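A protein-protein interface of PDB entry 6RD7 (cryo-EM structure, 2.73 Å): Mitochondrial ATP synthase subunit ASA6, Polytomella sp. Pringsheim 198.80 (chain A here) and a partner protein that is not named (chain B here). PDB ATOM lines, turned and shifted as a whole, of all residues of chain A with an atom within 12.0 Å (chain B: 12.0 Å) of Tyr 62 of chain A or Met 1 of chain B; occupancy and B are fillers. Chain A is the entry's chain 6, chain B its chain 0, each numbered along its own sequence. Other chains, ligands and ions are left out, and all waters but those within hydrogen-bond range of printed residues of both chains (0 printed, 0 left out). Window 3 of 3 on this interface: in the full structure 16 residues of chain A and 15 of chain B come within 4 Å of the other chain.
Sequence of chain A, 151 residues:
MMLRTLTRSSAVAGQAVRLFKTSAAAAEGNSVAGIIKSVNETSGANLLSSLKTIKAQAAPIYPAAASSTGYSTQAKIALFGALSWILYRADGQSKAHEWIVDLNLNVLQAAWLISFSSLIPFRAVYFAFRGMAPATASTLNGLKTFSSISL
The side-chain amino group (NZ) of Lys 9 of chain B lies within hydrogen-bond range of the backbone carbonyl oxygen (O) of Ala 64 of chain A, 2.7 Å away.
Hydrophobic or aromatic side chains of chain B that line the printed part of chain A: Met 1, Tyr 3 and Ala 5. Of the 14 printed residues of chain A, 6 touch a printed residue of chain B. Hydrophobic or aromatic side chains of chain A that line the printed part of chain B: Tyr 62, Pro 63 and Ala 66. Among the printed residues, 9 pairs touch across the chains.
No residue of chain B comes within 4 Å of Ala 59 of chain A. Of the printed residues of chain B, Ile 61 of chain A touches Tyr 3 (3.8 Å). Tyr 62 of chain A touches three residues of chain B. Of the printed residues of chain B, Pro 63 of chain A touches Ala 5 and Lys 9. Ala 64 of chain A touches one residue of chain B. Printed residues of chain B within 4 Å of Ala 65 of chain A: Ala 5 (3.8 Å). Of the printed residues of chain B, Ala 66 of chain A touches Lys 9 (3.4 Å). Of chain A, only Tyr 62 comes within 4 Å of Met 1 of chain B. Ser 2 of chain B touches just one residue of chain A: Tyr 62. Of chain A, only Ile 61 (3.8 Å) and Tyr 62 (3.6 Å) come within 4 Å of Tyr 3 of chain B. No residue of chain A comes within 4 Å of Ser 4 of chain B. Ala 5 of chain B touches two residues of chain A. Of the printed residues of chain A, Lys 9 of chain B touches Pro 63, Ala 64 and Ala 66. The nearest residue of chain A that does not touch Met 1 of chain B is Pro 63 of chain A (4.3 Å). The nearest printed residue of chain A that does not touch Lys 9 of chain B is Ala 65 of chain A (4.6 Å).
N of Ser 4 of chain B is in hydrogen-bond range of OG of Ser 2 of chain B.
Among the printed residues, merely in contact across the chains: Tyr 62 of chain A with Ser 2 of chain B (3.3 Å), Pro 63 of chain A with Ala 5 of chain B (3.3 Å), Ala 66 of chain A with Lys 9 of chain B (3.4 Å), Tyr 62 of chain A with Met 1 of chain B (3.6 Å), Tyr 62 of chain A with Tyr 3 of chain B (3.6 Å), Pro 63 of chain A with Lys 9 of chain B (3.7 Å), Ile 61 of chain A with Tyr 3 of chain B (3.8 Å) and Ala 65 of chain A with Ala 5 of chain B (3.8 Å).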
ATOM      1  N   GLU A  28     -29.457 -32.727  27.765  1.00  0.00           N
ATOM      2  CA  GLU A  28     -30.897 -32.573  27.929  1.00  0.00           C
ATOM      3  C   GLU A  28     -31.620 -33.857  27.539  1.00  0.00           C
ATOM      4  O   GLU A  28     -30.983 -34.843  27.165  1.00  0.00           O
ATOM      5  CB  GLU A  28     -31.407 -31.399  27.091  1.00  0.00           C
ATOM      6  CG  GLU A  28     -31.366 -31.632  25.589  1.00  0.00           C
ATOM      7  CD  GLU A  28     -30.082 -31.147  24.941  1.00  0.00           C
ATOM      8  OE1 GLU A  28     -29.099 -30.887  25.663  1.00  0.00           O
ATOM      9  OE2 GLU A  28     -30.061 -31.022  23.700  1.00  0.00           O
ATOM     10  N   SER A  31     -34.759 -35.718  21.695  1.00  0.00           N
ATOM     11  CA  SER A  31     -35.681 -34.916  20.899  1.00  0.00           C
ATOM     12  C   SER A  31     -36.880 -35.728  20.439  1.00  0.00           C
ATOM     13  O   SER A  31     -37.956 -35.173  20.194  1.00  0.00           O
ATOM     14  CB  SER A  31     -34.952 -34.325  19.696  1.00  0.00           C
ATOM     15  OG  SER A  31     -34.568 -35.338  18.785  1.00  0.00           O
ATOM     16  N   LYS A  55     -41.325 -29.573  15.064  1.00  0.00           N
ATOM     17  CA  LYS A  55     -40.112 -29.818  14.290  1.00  0.00           C
ATOM     18  C   LYS A  55     -39.001 -28.851  14.668  1.00  0.00           C
ATOM     19  O   LYS A  55     -37.848 -29.263  14.852  1.00  0.00           O
ATOM     20  CB  LYS A  55     -40.422 -29.694  12.801  1.00  0.00           C
ATOM     21  CG  LYS A  55     -39.292 -30.094  11.891  1.00  0.00           C
ATOM     22  CD  LYS A  55     -39.688 -29.925  10.442  1.00  0.00           C
ATOM     23  CE  LYS A  55     -38.536 -30.281   9.525  1.00  0.00           C
ATOM     24  NZ  LYS A  55     -38.163 -31.713   9.668  1.00  0.00           N
ATOM     25  N   ALA A  56     -39.345 -27.576  14.864  1.00  0.00           N
ATOM     26  CA  ALA A  56     -38.336 -26.586  15.217  1.00  0.00           C
ATOM     27  C   ALA A  56     -37.843 -26.781  16.642  1.00  0.00           C
ATOM     28  O   ALA A  56     -36.754 -26.317  16.997  1.00  0.00           O
ATOM     29  CB  ALA A  56     -38.894 -25.179  15.028  1.00  0.00           C
ATOM     30  N   GLN A  57     -38.620 -27.477  17.476  1.00  0.00           N
ATOM     31  CA  GLN A  57     -38.137 -27.766  18.818  1.00  0.00           C
ATOM     32  C   GLN A  57     -37.351 -29.068  18.840  1.00  0.00           C
ATOM     33  O   GLN A  57     -36.712 -29.401  19.844  1.00  0.00           O
ATOM     34  CB  GLN A  57     -39.301 -27.814  19.801  1.00  0.00           C
ATOM     35  CG  GLN A  57     -40.064 -26.509  19.886  1.00  0.00           C
ATOM     36  CD  GLN A  57     -41.313 -26.618  20.731  1.00  0.00           C
ATOM     37  OE1 GLN A  57     -42.224 -27.382  20.418  1.00  0.00           O
ATOM     38  NE2 GLN A  57     -41.365 -25.847  21.811  1.00  0.00           N
ATOM     39  N   ALA A  58     -37.378 -29.813  17.737  1.00  0.00           N
ATOM     40  CA  ALA A  58     -36.603 -31.043  17.674  1.00  0.00           C
ATOM     41  C   ALA A  58     -35.393 -30.899  16.775  1.00  0.00           C
ATOM     42  O   ALA A  58     -34.595 -31.835  16.665  1.00  0.00           O
ATOM     43  CB  ALA A  58     -37.471 -32.188  17.181  1.00  0.00           C
ATOM     44  N   ALA A  59     -35.266 -29.762  16.107  1.00  0.00           N
ATOM     45  CA  ALA A  59     -34.112 -29.509  15.267  1.00  0.00           C
ATOM     46  C   ALA A  59     -32.868 -29.376  16.139  1.00  0.00           C
ATOM     47  O   ALA A  59     -32.952 -28.850  17.255  1.00  0.00           O
ATOM     48  CB  ALA A  59     -34.326 -28.237  14.445  1.00  0.00           C
ATOM     49  N   PRO A  60     -31.714 -29.865  15.686  1.00  0.00           N
ATOM     50  CA  PRO A  60     -30.503 -29.758  16.502  1.00  0.00           C
ATOM     51  C   PRO A  60     -30.027 -28.320  16.578  1.00  0.00           C
ATOM     52  O   PRO A  60     -30.309 -27.505  15.699  1.00  0.00           O
ATOM     53  CB  PRO A  60     -29.494 -30.641  15.758  1.00  0.00           C
ATOM     54  CG  PRO A  60     -30.305 -31.446  14.798  1.00  0.00           C
ATOM     55  CD  PRO A  60     -31.464 -30.601  14.440  1.00  0.00           C
ATOM     56  N   ILE A  61     -29.316 -28.000  17.658  1.00  0.00           N
ATOM     57  CA  ILE A  61     -28.787 -26.649  17.806  1.00  0.00           C
ATOM     58  C   ILE A  61     -27.596 -26.531  16.860  1.00  0.00           C
ATOM     59  O   ILE A  61     -26.666 -27.338  16.876  1.00  0.00           O
ATOM     60  CB  ILE A  61     -28.428 -26.301  19.257  1.00  0.00           C
ATOM     61  CG1 ILE A  61     -27.816 -24.905  19.334  1.00  0.00           C
ATOM     62  CG2 ILE A  61     -27.519 -27.325  19.932  1.00  0.00           C
ATOM     63  CD1 ILE A  61     -28.780 -23.806  18.981  1.00  0.00           C
ATOM     64  N   TYR A  62     -27.679 -25.580  15.965  1.00  0.00           N
ATOM     65  CA  TYR A  62     -26.532 -25.200  15.171  1.00  0.00           C
ATOM     66  C   TYR A  62     -26.228 -23.766  15.567  1.00  0.00           C
ATOM     67  O   TYR A  62     -26.975 -22.860  15.177  1.00  0.00           O
ATOM     68  CB  TYR A  62     -26.816 -25.303  13.680  1.00  0.00           C
ATOM     69  CG  TYR A  62     -27.275 -26.645  13.172  1.00  0.00           C
ATOM     70  CD1 TYR A  62     -26.403 -27.720  13.099  1.00  0.00           C
ATOM     71  CD2 TYR A  62     -28.572 -26.824  12.718  1.00  0.00           C
ATOM     72  CE1 TYR A  62     -26.818 -28.941  12.614  1.00  0.00           C
ATOM     73  CE2 TYR A  62     -28.995 -28.041  12.232  1.00  0.00           C
ATOM     74  CZ  TYR A  62     -28.114 -29.094  12.184  1.00  0.00           C
ATOM     75  OH  TYR A  62     -28.533 -30.308  11.699  1.00  0.00           O
ATOM     76  N   PRO A  63     -25.176 -23.531  16.367  1.00  0.00           N
ATOM     77  CA  PRO A  63     -24.954 -22.207  16.965  1.00  0.00           C
ATOM     78  C   PRO A  63     -24.719 -21.091  15.964  1.00  0.00           C
ATOM     79  O   PRO A  63     -23.938 -21.242  15.022  1.00  0.00           O
ATOM     80  CB  PRO A  63     -23.715 -22.433  17.838  1.00  0.00           C
ATOM     81  CG  PRO A  63     -23.735 -23.878  18.140  1.00  0.00           C
ATOM     82  CD  PRO A  63     -24.240 -24.531  16.903  1.00  0.00           C
ATOM     83  N   ALA A  64     -25.430 -19.983  16.147  1.00  0.00           N
ATOM     84  CA  ALA A  64     -25.305 -18.844  15.253  1.00  0.00           C
ATOM     85  C   ALA A  64     -23.961 -18.162  15.455  1.00  0.00           C
ATOM     86  O   ALA A  64     -23.316 -18.317  16.493  1.00  0.00           O
ATOM     87  CB  ALA A  64     -26.439 -17.851  15.490  1.00  0.00           C
ATOM     88  N   ALA A  65     -23.544 -17.407  14.439  1.00  0.00           N
ATOM     89  CA  ALA A  65     -22.227 -16.780  14.438  1.00  0.00           C
ATOM     90  C   ALA A  65     -22.136 -15.712  15.519  1.00  0.00           C
ATOM     91  O   ALA A  65     -22.859 -14.712  15.481  1.00  0.00           O
ATOM     92  CB  ALA A  65     -21.937 -16.179  13.065  1.00  0.00           C
ATOM     93  N   ALA A  66     -21.244 -15.933  16.479  1.00  0.00           N
ATOM     94  CA  ALA A  66     -21.112 -15.089  17.651  1.00  0.00           C
ATOM     95  C   ALA A  66     -20.225 -13.885  17.352  1.00  0.00           C
ATOM     96  O   ALA A  66     -19.960 -13.543  16.196  1.00  0.00           O
ATOM     97  CB  ALA A  66     -20.562 -15.889  18.829  1.00  0.00           C
ATOM     98  N   MET B   1     -28.814 -25.570   8.012  1.00  0.00           N
ATOM     99  CA  MET B   1     -27.870 -24.846   8.852  1.00  0.00           C
ATOM    100  C   MET B   1     -26.758 -25.812   9.268  1.00  0.00           C
ATOM    101  O   MET B   1     -26.962 -27.022   9.309  1.00  0.00           O
ATOM    102  CB  MET B   1     -28.600 -24.216  10.049  1.00  0.00           C
ATOM    103  CG  MET B   1     -27.787 -23.247  10.901  1.00  0.00           C
ATOM    104  SD  MET B   1     -27.103 -21.811  10.066  1.00  0.00           S
ATOM    105  CE  MET B   1     -25.751 -21.424  11.179  1.00  0.00           C
ATOM    106  N   SER B   2     -25.577 -25.264   9.545  1.00  0.00           N
ATOM    107  CA  SER B   2     -24.350 -26.038   9.646  1.00  0.00           C
ATOM    108  C   SER B   2     -23.680 -25.862  10.999  1.00  0.00           C
ATOM    109  O   SER B   2     -24.128 -25.061  11.821  1.00  0.00           O
ATOM    110  CB  SER B   2     -23.394 -25.612   8.534  1.00  0.00           C
ATOM    111  OG  SER B   2     -22.923 -24.297   8.769  1.00  0.00           O
ATOM    112  N   TYR B   3     -22.603 -26.603  11.241  1.00  0.00           N
ATOM    113  CA  TYR B   3     -21.758 -26.383  12.402  1.00  0.00           C
ATOM    114  C   TYR B   3     -20.578 -25.482  12.088  1.00  0.00           C
ATOM    115  O   TYR B   3     -19.597 -25.486  12.832  1.00  0.00           O
ATOM    116  CB  TYR B   3     -21.243 -27.710  12.952  1.00  0.00           C
ATOM    117  CG  TYR B   3     -22.277 -28.594  13.594  1.00  0.00           C
ATOM    118  CD1 TYR B   3     -22.754 -28.322  14.864  1.00  0.00           C
ATOM    119  CD2 TYR B   3     -22.754 -29.719  12.942  1.00  0.00           C
ATOM    120  CE1 TYR B   3     -23.690 -29.135  15.458  1.00  0.00           C
ATOM    121  CE2 TYR B   3     -23.689 -30.539  13.531  1.00  0.00           C
ATOM    122  CZ  TYR B   3     -24.152 -30.240  14.788  1.00  0.00           C
ATOM    123  OH  TYR B   3     -25.086 -31.047  15.386  1.00  0.00           O
ATOM    124  N   SER B   4     -20.651 -24.714  10.999  1.00  0.00           N
ATOM    125  CA  SER B   4     -19.516 -23.914  10.552  1.00  0.00           C
ATOM    126  C   SER B   4     -19.251 -22.749  11.492  1.00  0.00           C
ATOM    127  O   SER B   4     -18.096 -22.406  11.766  1.00  0.00           O
ATOM    128  CB  SER B   4     -19.770 -23.402   9.137  1.00  0.00           C
ATOM    129  OG  SER B   4     -19.754 -24.463   8.204  1.00  0.00           O
ATOM    130  N   ALA B   5     -20.316 -22.122  11.994  1.00  0.00           N
ATOM    131  CA  ALA B   5     -20.152 -20.984  12.887  1.00  0.00           C
ATOM    132  C   ALA B   5     -19.636 -21.421  14.249  1.00  0.00           C
ATOM    133  O   ALA B   5     -18.913 -20.672  14.919  1.00  0.00           O
ATOM    134  CB  ALA B   5     -21.473 -20.236  13.026  1.00  0.00           C
ATOM    135  N   TYR B   6     -19.981 -22.642  14.662  1.00  0.00           N
ATOM    136  CA  TYR B   6     -19.487 -23.181  15.923  1.00  0.00           C
ATOM    137  C   TYR B   6     -17.983 -23.413  15.867  1.00  0.00           C
ATOM    138  O   TYR B   6     -17.277 -23.230  16.864  1.00  0.00           O
ATOM    139  CB  TYR B   6     -20.225 -24.479  16.251  1.00  0.00           C
ATOM    140  CG  TYR B   6     -19.557 -25.319  17.306  1.00  0.00           C
ATOM    141  CD1 TYR B   6     -19.587 -24.940  18.638  1.00  0.00           C
ATOM    142  CD2 TYR B   6     -18.898 -26.493  16.973  1.00  0.00           C
ATOM    143  CE1 TYR B   6     -18.979 -25.702  19.606  1.00  0.00           C
ATOM    144  CE2 TYR B   6     -18.284 -27.258  17.932  1.00  0.00           C
ATOM    145  CZ  TYR B   6     -18.329 -26.859  19.248  1.00  0.00           C
ATOM    146  OH  TYR B   6     -17.719 -27.624  20.211  1.00  0.00           O
ATOM    147  N   PHE B   7     -17.474 -23.809  14.702  1.00  0.00           N
ATOM    148  CA  PHE B   7     -16.038 -24.009  14.566  1.00  0.00           C
ATOM    149  C   PHE B   7     -15.330 -22.703  14.257  1.00  0.00           C
ATOM    150  O   PHE B   7     -14.122 -22.576  14.482  1.00  0.00           O
ATOM    151  CB  PHE B   7     -15.755 -25.054  13.493  1.00  0.00           C
ATOM    152  CG  PHE B   7     -16.028 -26.437  13.948  1.00  0.00           C
ATOM    153  CD1 PHE B   7     -15.381 -26.940  15.059  1.00  0.00           C
ATOM    154  CD2 PHE B   7     -16.955 -27.223  13.302  1.00  0.00           C
ATOM    155  CE1 PHE B   7     -15.641 -28.206  15.503  1.00  0.00           C
ATOM    156  CE2 PHE B   7     -17.218 -28.488  13.743  1.00  0.00           C
ATOM    157  CZ  PHE B   7     -16.564 -28.975  14.846  1.00  0.00           C
ATOM    158  N   ALA B   8     -16.066 -21.716  13.745  1.00  0.00           N
ATOM    159  CA  ALA B   8     -15.490 -20.388  13.584  1.00  0.00           C
ATOM    160  C   ALA B   8     -15.393 -19.661  14.917  1.00  0.00           C
ATOM    161  O   ALA B   8     -14.612 -18.713  15.044  1.00  0.00           O
ATOM    162  CB  ALA B   8     -16.315 -19.577  12.590  1.00  0.00           C
ATOM    163  N   LYS B   9     -16.183 -20.079  15.911  1.00  0.00           N
ATOM    164  CA  LYS B   9     -16.101 -19.469  17.237  1.00  0.00           C
ATOM    165  C   LYS B   9     -14.770 -19.768  17.912  1.00  0.00           C
ATOM    166  O   LYS B   9     -14.224 -18.917  18.623  1.00  0.00           O
ATOM    167  CB  LYS B   9     -17.239 -19.961  18.124  1.00  0.00           C
ATOM    168  CG  LYS B   9     -18.563 -19.286  17.896  1.00  0.00           C
ATOM    169  CD  LYS B   9     -19.623 -19.949  18.744  1.00  0.00           C
ATOM    170  CE  LYS B   9     -20.961 -19.937  18.051  1.00  0.00           C
ATOM    171  NZ  LYS B   9     -21.928 -19.025  18.714  1.00  0.00           N
